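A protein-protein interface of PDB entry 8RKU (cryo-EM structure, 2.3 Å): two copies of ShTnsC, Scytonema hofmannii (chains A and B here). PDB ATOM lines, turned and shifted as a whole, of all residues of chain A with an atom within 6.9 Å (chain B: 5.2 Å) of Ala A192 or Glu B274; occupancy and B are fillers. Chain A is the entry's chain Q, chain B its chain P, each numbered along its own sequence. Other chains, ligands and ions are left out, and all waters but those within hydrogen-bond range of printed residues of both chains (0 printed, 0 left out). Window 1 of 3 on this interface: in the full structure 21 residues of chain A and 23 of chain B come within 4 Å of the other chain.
No position is printed for both chains.
Among the printed residues, pairs that only touch across the chains: Trp A45 with Arg B254 (3.995 Å), Lys A49 with Arg B254 (3.8 Å), Arg A191 with Glu B274 (3.9 Å), Arg A191 with Tyr B275 (3.0 Å), Ala A192 with Glu B274 (3.6 Å), Ala A192 with Tyr B275 (3.5 Å) and His A193 with Tyr B275 (3.5 Å).
The backbone carbonyl oxygen of Lys A49 is in hydrogen-bond range of the backbone NH of Lys A54, at 3.2 Å.
The guanidinium group (NH1) of Arg B254 is in salt-bridge range of the side-chain carboxylate (OE2) of Glu B274 (3.0 Å).
The guanidinium group of Arg B254 is in salt-bridge range of the side-chain carboxylate of Glu B270 (2.5 Å).
NH1 of Arg A57 sits at hydrogen-bond distance from O of Arg A191, 2.8 Å away.
The side-chain carboxylate (OE2) of Glu B250 lies within salt-bridge range of the guanidinium group (NH2) of Arg B254.
N of Arg A57 is in hydrogen-bond range of O of Ala A192, at 2.9 Å.
OE1 of Glu B250 lies within salt-bridge range of NZ of Lys A54, at 2.8 Å.
The side-chain carboxylate (OE2) of Glu B250 lies within salt-bridge range of the side-chain amino group (NZ) of Lys A49, at 2.8 Å.
O of Glu B274 is in hydrogen-bond range of N of His A193.
The side-chain amino group (NZ) of Lys A49 is in salt-bridge range of the side-chain carboxylate (OE1) of Glu B274 (2.7 Å).
The indole nitrogen (NE1) of Trp A45 sits at hydrogen-bond distance from the side-chain carboxylate (OE1) of Glu B274, 3.2 Å away.
Of chain A, only Trp A45 (3.2 Å), Lys A49 (2.7 Å), Arg A191 (3.9 Å), Ala A192 (3.6 Å) and His A193 (2.9 Å) come within 4 Å of Glu B274.
Printed residues of chain B within 4 Å of Lys A49: Glu B250 (2.8 Å), Arg B254 (3.8 Å) and Glu B274 (2.7 Å).
Of the printed residues of chain B, Lys A54 touches Glu B250.
Of the printed residues of chain A, Tyr B275 touches Arg A191 (3.0 Å), Ala A192 (3.5 Å) and His A193 (3.5 Å).
Of the printed residues of chain A, Arg B254 touches Trp A45 and Lys A49.
Val A58 touches none of the printed residues of chain B.
The nearest printed residue of chain B that does not touch Ala A192 is Glu B250 (6.2 Å).
The nearest residue of chain A that does not touch Glu B274 is Leu A194 (5.3 Å).
Of the 8 printed residues of chain B, 4 touch a printed residue of chain A.
Printed residues of chain B that touch a printed residue of chain A: Glu B250, Arg B254, Glu B274 and Tyr B275.
Hydrophobic or aromatic side chains of chain A that line the printed part of chain B: Trp A45, Ala A192 and His A193.
Among the printed residues, 12 pairs touch across the chains.
Among the printed residues, Asp or Glu carboxylates within 4 Å of a Lys or Arg side-chain nitrogen of the other chain: Lys A49 with Glu B250 (2.8 Å), Lys A49 with Glu B274 (2.7 Å) and Lys A54 with Glu B250 (2.8 Å).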
ATOM      1  N   TRP A  45     -11.899 -11.155  11.494  1.00  0.00           N
ATOM      2  CA  TRP A  45     -12.605 -12.431  11.457  1.00  0.00           C
ATOM      3  C   TRP A  45     -13.299 -12.740  12.785  1.00  0.00           C
ATOM      4  O   TRP A  45     -14.488 -13.086  12.809  1.00  0.00           O
ATOM      5  CB  TRP A  45     -11.607 -13.520  11.060  1.00  0.00           C
ATOM      6  CG  TRP A  45     -12.171 -14.848  10.650  1.00  0.00           C
ATOM      7  CD1 TRP A  45     -12.799 -15.138   9.475  1.00  0.00           C
ATOM      8  CD2 TRP A  45     -12.046 -16.091  11.353  1.00  0.00           C
ATOM      9  NE1 TRP A  45     -13.132 -16.468   9.432  1.00  0.00           N
ATOM     10  CE2 TRP A  45     -12.676 -17.077  10.569  1.00  0.00           C
ATOM     11  CE3 TRP A  45     -11.492 -16.461  12.580  1.00  0.00           C
ATOM     12  CZ2 TRP A  45     -12.761 -18.407  10.972  1.00  0.00           C
ATOM     13  CZ3 TRP A  45     -11.581 -17.776  12.977  1.00  0.00           C
ATOM     14  CH2 TRP A  45     -12.210 -18.735  12.176  1.00  0.00           C
ATOM     15  N   LYS A  49     -17.146 -13.274  13.474  1.00  0.00           N
ATOM     16  CA  LYS A  49     -17.632 -14.528  14.038  1.00  0.00           C
ATOM     17  C   LYS A  49     -18.382 -14.311  15.349  1.00  0.00           C
ATOM     18  O   LYS A  49     -19.440 -14.910  15.571  1.00  0.00           O
ATOM     19  CB  LYS A  49     -16.461 -15.481  14.254  1.00  0.00           C
ATOM     20  CG  LYS A  49     -16.851 -16.931  14.229  1.00  0.00           C
ATOM     21  CD  LYS A  49     -17.160 -17.367  12.812  1.00  0.00           C
ATOM     22  CE  LYS A  49     -15.901 -17.325  11.959  1.00  0.00           C
ATOM     23  NZ  LYS A  49     -16.152 -17.730  10.550  1.00  0.00           N
ATOM     24  N   LYS A  54     -21.068 -17.682  15.808  1.00  0.00           N
ATOM     25  CA  LYS A  54     -20.630 -18.993  15.349  1.00  0.00           C
ATOM     26  C   LYS A  54     -19.438 -19.463  16.176  1.00  0.00           C
ATOM     27  O   LYS A  54     -18.639 -18.663  16.662  1.00  0.00           O
ATOM     28  CB  LYS A  54     -20.287 -18.967  13.862  1.00  0.00           C
ATOM     29  CG  LYS A  54     -21.419 -19.462  12.981  1.00  0.00           C
ATOM     30  CD  LYS A  54     -22.558 -18.460  12.896  1.00  0.00           C
ATOM     31  CE  LYS A  54     -23.527 -18.817  11.774  1.00  0.00           C
ATOM     32  NZ  LYS A  54     -22.869 -18.791  10.442  1.00  0.00           N
ATOM     33  N   SER A  55     -19.315 -20.775  16.317  1.00  0.00           N
ATOM     34  CA  SER A  55     -18.085 -21.404  16.773  1.00  0.00           C
ATOM     35  C   SER A  55     -17.144 -21.706  15.616  1.00  0.00           C
ATOM     36  O   SER A  55     -17.569 -21.890  14.472  1.00  0.00           O
ATOM     37  CB  SER A  55     -18.400 -22.696  17.529  1.00  0.00           C
ATOM     38  OG  SER A  55     -18.714 -22.433  18.884  1.00  0.00           O
ATOM     39  N   CYS A  56     -15.856 -21.754  15.927  1.00  0.00           N
ATOM     40  CA  CYS A  56     -14.816 -21.948  14.923  1.00  0.00           C
ATOM     41  C   CYS A  56     -13.522 -22.324  15.634  1.00  0.00           C
ATOM     42  O   CYS A  56     -13.461 -22.395  16.863  1.00  0.00           O
ATOM     43  CB  CYS A  56     -14.648 -20.692  14.068  1.00  0.00           C
ATOM     44  SG  CYS A  56     -13.989 -19.282  14.979  1.00  0.00           S
ATOM     45  N   ARG A  57     -12.479 -22.562  14.841  1.00  0.00           N
ATOM     46  CA  ARG A  57     -11.138 -22.804  15.345  1.00  0.00           C
ATOM     47  C   ARG A  57     -10.103 -21.971  14.603  1.00  0.00           C
ATOM     48  O   ARG A  57     -10.286 -21.607  13.440  1.00  0.00           O
ATOM     49  CB  ARG A  57     -10.802 -24.303  15.276  1.00  0.00           C
ATOM     50  CG  ARG A  57     -10.708 -24.881  13.878  1.00  0.00           C
ATOM     51  CD  ARG A  57     -10.525 -26.393  13.957  1.00  0.00           C
ATOM     52  NE  ARG A  57     -10.008 -26.986  12.731  1.00  0.00           N
ATOM     53  CZ  ARG A  57     -10.657 -27.009  11.575  1.00  0.00           C
ATOM     54  NH1 ARG A  57     -11.905 -26.584  11.472  1.00  0.00           N
ATOM     55  NH2 ARG A  57     -10.052 -27.505  10.503  1.00  0.00           N
ATOM     56  N   VAL A  58      -9.021 -21.653  15.309  1.00  0.00           N
ATOM     57  CA  VAL A  58      -7.877 -20.922  14.773  1.00  0.00           C
ATOM     58  C   VAL A  58      -6.662 -21.835  14.872  1.00  0.00           C
ATOM     59  O   VAL A  58      -6.306 -22.280  15.972  1.00  0.00           O
ATOM     60  CB  VAL A  58      -7.638 -19.603  15.524  1.00  0.00           C
ATOM     61  CG1 VAL A  58      -6.476 -18.846  14.918  1.00  0.00           C
ATOM     62  CG2 VAL A  58      -8.896 -18.752  15.516  1.00  0.00           C
ATOM     63  N   VAL A  59      -6.033 -22.121  13.731  1.00  0.00           N
ATOM     64  CA  VAL A  59      -5.090 -23.229  13.607  1.00  0.00           C
ATOM     65  C   VAL A  59      -3.763 -22.718  13.064  1.00  0.00           C
ATOM     66  O   VAL A  59      -3.730 -22.020  12.045  1.00  0.00           O
ATOM     67  CB  VAL A  59      -5.637 -24.343  12.695  1.00  0.00           C
ATOM     68  CG1 VAL A  59      -4.743 -25.568  12.771  1.00  0.00           C
ATOM     69  CG2 VAL A  59      -7.065 -24.694  13.072  1.00  0.00           C
ATOM     70  N   LEU A 187     -15.902 -32.153  15.556  1.00  0.00           N
ATOM     71  CA  LEU A 187     -15.497 -31.860  14.184  1.00  0.00           C
ATOM     72  C   LEU A 187     -16.535 -31.044  13.425  1.00  0.00           C
ATOM     73  O   LEU A 187     -16.223 -29.982  12.877  1.00  0.00           O
ATOM     74  CB  LEU A 187     -15.223 -33.170  13.446  1.00  0.00           C
ATOM     75  CG  LEU A 187     -14.966 -33.095  11.939  1.00  0.00           C
ATOM     76  CD1 LEU A 187     -13.732 -32.291  11.619  1.00  0.00           C
ATOM     77  CD2 LEU A 187     -14.856 -34.493  11.359  1.00  0.00           C
ATOM     78  N   GLU A 188     -17.773 -31.518  13.382  1.00  0.00           N
ATOM     79  CA  GLU A 188     -18.790 -30.859  12.575  1.00  0.00           C
ATOM     80  C   GLU A 188     -19.327 -29.571  13.184  1.00  0.00           C
ATOM     81  O   GLU A 188     -20.034 -28.832  12.493  1.00  0.00           O
ATOM     82  CB  GLU A 188     -19.933 -31.833  12.300  1.00  0.00           C
ATOM     83  CG  GLU A 188     -19.495 -33.073  11.540  1.00  0.00           C
ATOM     84  CD  GLU A 188     -19.041 -32.782  10.118  1.00  0.00           C
ATOM     85  OE1 GLU A 188     -19.119 -31.616   9.676  1.00  0.00           O
ATOM     86  OE2 GLU A 188     -18.591 -33.732   9.442  1.00  0.00           O
ATOM     87  N   ARG A 189     -19.018 -29.282  14.444  1.00  0.00           N
ATOM     88  CA  ARG A 189     -19.304 -27.979  15.035  1.00  0.00           C
ATOM     89  C   ARG A 189     -18.199 -26.960  14.773  1.00  0.00           C
ATOM     90  O   ARG A 189     -18.485 -25.789  14.509  1.00  0.00           O
ATOM     91  CB  ARG A 189     -19.549 -28.123  16.537  1.00  0.00           C
ATOM     92  CG  ARG A 189     -20.950 -28.604  16.862  1.00  0.00           C
ATOM     93  CD  ARG A 189     -21.095 -28.967  18.325  1.00  0.00           C
ATOM     94  NE  ARG A 189     -22.439 -29.447  18.628  1.00  0.00           N
ATOM     95  CZ  ARG A 189     -22.954 -30.588  18.192  1.00  0.00           C
ATOM     96  NH1 ARG A 189     -22.238 -31.447  17.486  1.00  0.00           N
ATOM     97  NH2 ARG A 189     -24.216 -30.881  18.487  1.00  0.00           N
ATOM     98  N   PHE A 190     -16.941 -27.387  14.858  1.00  0.00           N
ATOM     99  CA  PHE A 190     -15.770 -26.527  14.736  1.00  0.00           C
ATOM    100  C   PHE A 190     -15.116 -26.640  13.360  1.00  0.00           C
ATOM    101  O   PHE A 190     -13.907 -26.441  13.216  1.00  0.00           O
ATOM    102  CB  PHE A 190     -14.786 -26.818  15.863  1.00  0.00           C
ATOM    103  CG  PHE A 190     -15.334 -26.483  17.216  1.00  0.00           C
ATOM    104  CD1 PHE A 190     -15.331 -25.173  17.666  1.00  0.00           C
ATOM    105  CD2 PHE A 190     -15.866 -27.465  18.031  1.00  0.00           C
ATOM    106  CE1 PHE A 190     -15.842 -24.849  18.901  1.00  0.00           C
ATOM    107  CE2 PHE A 190     -16.379 -27.147  19.272  1.00  0.00           C
ATOM    108  CZ  PHE A 190     -16.364 -25.836  19.708  1.00  0.00           C
ATOM    109  N   ARG A 191     -15.916 -26.980  12.350  1.00  0.00           N
ATOM    110  CA  ARG A 191     -15.439 -27.131  10.980  1.00  0.00           C
ATOM    111  C   ARG A 191     -14.871 -25.827  10.419  1.00  0.00           C
ATOM    112  O   ARG A 191     -13.873 -25.844   9.690  1.00  0.00           O
ATOM    113  CB  ARG A 191     -16.597 -27.644  10.125  1.00  0.00           C
ATOM    114  CG  ARG A 191     -16.341 -27.826   8.650  1.00  0.00           C
ATOM    115  CD  ARG A 191     -17.629 -28.311   8.010  1.00  0.00           C
ATOM    116  NE  ARG A 191     -18.748 -27.440   8.349  1.00  0.00           N
ATOM    117  CZ  ARG A 191     -19.061 -26.323   7.705  1.00  0.00           C
ATOM    118  NH1 ARG A 191     -18.552 -26.047   6.520  1.00  0.00           N
ATOM    119  NH2 ARG A 191     -19.966 -25.503   8.231  1.00  0.00           N
ATOM    120  N   ALA A 192     -15.494 -24.693  10.735  1.00  0.00           N
ATOM    121  CA  ALA A 192     -14.972 -23.396  10.316  1.00  0.00           C
ATOM    122  C   ALA A 192     -13.602 -23.139  10.938  1.00  0.00           C
ATOM    123  O   ALA A 192     -13.420 -23.274  12.150  1.00  0.00           O
ATOM    124  CB  ALA A 192     -15.943 -22.281  10.701  1.00  0.00           C
ATOM    125  N   HIS A 193     -12.636 -22.764  10.101  1.00  0.00           N
ATOM    126  CA  HIS A 193     -11.281 -22.507  10.565  1.00  0.00           C
ATOM    127  C   HIS A 193     -10.690 -21.304   9.847  1.00  0.00           C
ATOM    128  O   HIS A 193     -11.067 -20.981   8.717  1.00  0.00           O
ATOM    129  CB  HIS A 193     -10.371 -23.717  10.331  1.00  0.00           C
ATOM    130  CG  HIS A 193     -10.066 -23.964   8.886  1.00  0.00           C
ATOM    131  ND1 HIS A 193      -9.007 -23.371   8.235  1.00  0.00           N
ATOM    132  CD2 HIS A 193     -10.697 -24.723   7.960  1.00  0.00           C
ATOM    133  CE1 HIS A 193      -8.992 -23.760   6.975  1.00  0.00           C
ATOM    134  NE2 HIS A 193     -10.008 -24.581   6.782  1.00  0.00           N
ATOM    135  N   LEU A 194      -9.741 -20.660  10.524  1.00  0.00           N
ATOM    136  CA  LEU A 194      -8.824 -19.688   9.945  1.00  0.00           C
ATOM    137  C   LEU A 194      -7.416 -20.263   9.918  1.00  0.00           C
ATOM    138  O   LEU A 194      -6.899 -20.702  10.952  1.00  0.00           O
ATOM    139  CB  LEU A 194      -8.839 -18.371  10.724  1.00  0.00           C
ATOM    140  CG  LEU A 194      -7.838 -17.322  10.230  1.00  0.00           C
ATOM    141  CD1 LEU A 194      -8.064 -17.032   8.773  1.00  0.00           C
ATOM    142  CD2 LEU A 194      -7.963 -16.047  11.035  1.00  0.00           C
ATOM    143  N   GLU B 250     -23.904 -17.134   7.674  1.00  0.00           N
ATOM    144  CA  GLU B 250     -22.614 -16.456   7.591  1.00  0.00           C
ATOM    145  C   GLU B 250     -22.580 -15.479   6.421  1.00  0.00           C
ATOM    146  O   GLU B 250     -22.195 -14.315   6.577  1.00  0.00           O
ATOM    147  CB  GLU B 250     -21.500 -17.494   7.455  1.00  0.00           C
ATOM    148  CG  GLU B 250     -20.090 -17.001   7.749  1.00  0.00           C
ATOM    149  CD  GLU B 250     -19.774 -16.935   9.227  1.00  0.00           C
ATOM    150  OE1 GLU B 250     -20.702 -17.092  10.044  1.00  0.00           O
ATOM    151  OE2 GLU B 250     -18.591 -16.742   9.574  1.00  0.00           O
ATOM    152  N   ARG B 254     -22.627 -11.265   6.476  1.00  0.00           N
ATOM    153  CA  ARG B 254     -21.578 -10.549   5.756  1.00  0.00           C
ATOM    154  C   ARG B 254     -22.148  -9.627   4.680  1.00  0.00           C
ATOM    155  O   ARG B 254     -21.768  -8.455   4.595  1.00  0.00           O
ATOM    156  CB  ARG B 254     -20.578 -11.542   5.164  1.00  0.00           C
ATOM    157  CG  ARG B 254     -19.705 -12.175   6.226  1.00  0.00           C
ATOM    158  CD  ARG B 254     -18.696 -13.143   5.659  1.00  0.00           C
ATOM    159  NE  ARG B 254     -18.064 -13.906   6.724  1.00  0.00           N
ATOM    160  CZ  ARG B 254     -16.907 -14.542   6.612  1.00  0.00           C
ATOM    161  NH1 ARG B 254     -16.117 -14.363   5.565  1.00  0.00           N
ATOM    162  NH2 ARG B 254     -16.496 -15.322   7.607  1.00  0.00           N
ATOM    163  N   GLU B 270     -16.512 -17.165  -0.481  1.00  0.00           N
ATOM    164  CA  GLU B 270     -15.631 -16.774   0.615  1.00  0.00           C
ATOM    165  C   GLU B 270     -15.997 -17.487   1.911  1.00  0.00           C
ATOM    166  O   GLU B 270     -15.115 -17.967   2.635  1.00  0.00           O
ATOM    167  CB  GLU B 270     -15.664 -15.256   0.801  1.00  0.00           C
ATOM    168  CG  GLU B 270     -14.783 -14.747   1.936  1.00  0.00           C
ATOM    169  CD  GLU B 270     -15.106 -13.318   2.343  1.00  0.00           C
ATOM    170  OE1 GLU B 270     -15.154 -12.439   1.459  1.00  0.00           O
ATOM    171  OE2 GLU B 270     -15.296 -13.069   3.550  1.00  0.00           O
ATOM    172  N   VAL B 271     -17.292 -17.560   2.228  1.00  0.00           N
ATOM    173  CA  VAL B 271     -17.742 -18.344   3.376  1.00  0.00           C
ATOM    174  C   VAL B 271     -17.424 -19.824   3.182  1.00  0.00           C
ATOM    175  O   VAL B 271     -16.809 -20.462   4.043  1.00  0.00           O
ATOM    176  CB  VAL B 271     -19.247 -18.123   3.616  1.00  0.00           C
ATOM    177  CG1 VAL B 271     -19.759 -19.079   4.678  1.00  0.00           C
ATOM    178  CG2 VAL B 271     -19.511 -16.687   4.027  1.00  0.00           C
ATOM    179  N   ALA B 272     -17.838 -20.386   2.045  1.00  0.00           N
ATOM    180  CA  ALA B 272     -17.599 -21.796   1.749  1.00  0.00           C
ATOM    181  C   ALA B 272     -16.119 -22.167   1.714  1.00  0.00           C
ATOM    182  O   ALA B 272     -15.791 -23.355   1.775  1.00  0.00           O
ATOM    183  CB  ALA B 272     -18.251 -22.165   0.416  1.00  0.00           C
ATOM    184  N   LYS B 273     -15.226 -21.185   1.621  1.00  0.00           N
ATOM    185  CA  LYS B 273     -13.785 -21.412   1.650  1.00  0.00           C
ATOM    186  C   LYS B 273     -13.208 -21.541   3.056  1.00  0.00           C
ATOM    187  O   LYS B 273     -12.050 -21.947   3.198  1.00  0.00           O
ATOM    188  CB  LYS B 273     -13.074 -20.282   0.894  1.00  0.00           C
ATOM    189  CG  LYS B 273     -11.598 -20.525   0.614  1.00  0.00           C
ATOM    190  CD  LYS B 273     -11.399 -21.813  -0.165  1.00  0.00           C
ATOM    191  CE  LYS B 273      -9.963 -21.971  -0.629  1.00  0.00           C
ATOM    192  NZ  LYS B 273      -9.046 -22.271   0.503  1.00  0.00           N
ATOM    193  N   GLU B 274     -13.979 -21.252   4.097  1.00  0.00           N
ATOM    194  CA  GLU B 274     -13.474 -21.317   5.463  1.00  0.00           C
ATOM    195  C   GLU B 274     -13.345 -22.746   6.008  1.00  0.00           C
ATOM    196  O   GLU B 274     -13.207 -22.915   7.224  1.00  0.00           O
ATOM    197  CB  GLU B 274     -14.365 -20.482   6.380  1.00  0.00           C
ATOM    198  CG  GLU B 274     -14.489 -19.036   5.934  1.00  0.00           C
ATOM    199  CD  GLU B 274     -14.897 -18.103   7.052  1.00  0.00           C
ATOM    200  OE1 GLU B 274     -15.159 -18.589   8.171  1.00  0.00           O
ATOM    201  OE2 GLU B 274     -14.957 -16.880   6.810  1.00  0.00           O
ATOM    202  N   TYR B 275     -13.381 -23.761   5.148  1.00  0.00           N
ATOM    203  CA  TYR B 275     -13.463 -25.158   5.577  1.00  0.00           C
ATOM    204  C   TYR B 275     -12.493 -26.048   4.800  1.00  0.00           C
ATOM    205  O   TYR B 275     -12.622 -26.238   3.591  1.00  0.00           O
ATOM    206  CB  TYR B 275     -14.887 -25.678   5.414  1.00  0.00           C
ATOM    207  CG  TYR B 275     -15.931 -24.673   5.813  1.00  0.00           C
ATOM    208  CD1 TYR B 275     -16.039 -24.246   7.126  1.00  0.00           C
ATOM    209  CD2 TYR B 275     -16.781 -24.117   4.872  1.00  0.00           C
ATOM    210  CE1 TYR B 275     -16.991 -23.329   7.499  1.00  0.00           C
ATOM    211  CE2 TYR B 275     -17.727 -23.190   5.238  1.00  0.00           C
ATOM    212  CZ  TYR B 275     -17.831 -22.800   6.554  1.00  0.00           C
ATOM    213  OH  TYR B 275     -18.770 -21.869   6.932  1.00  0.00           O
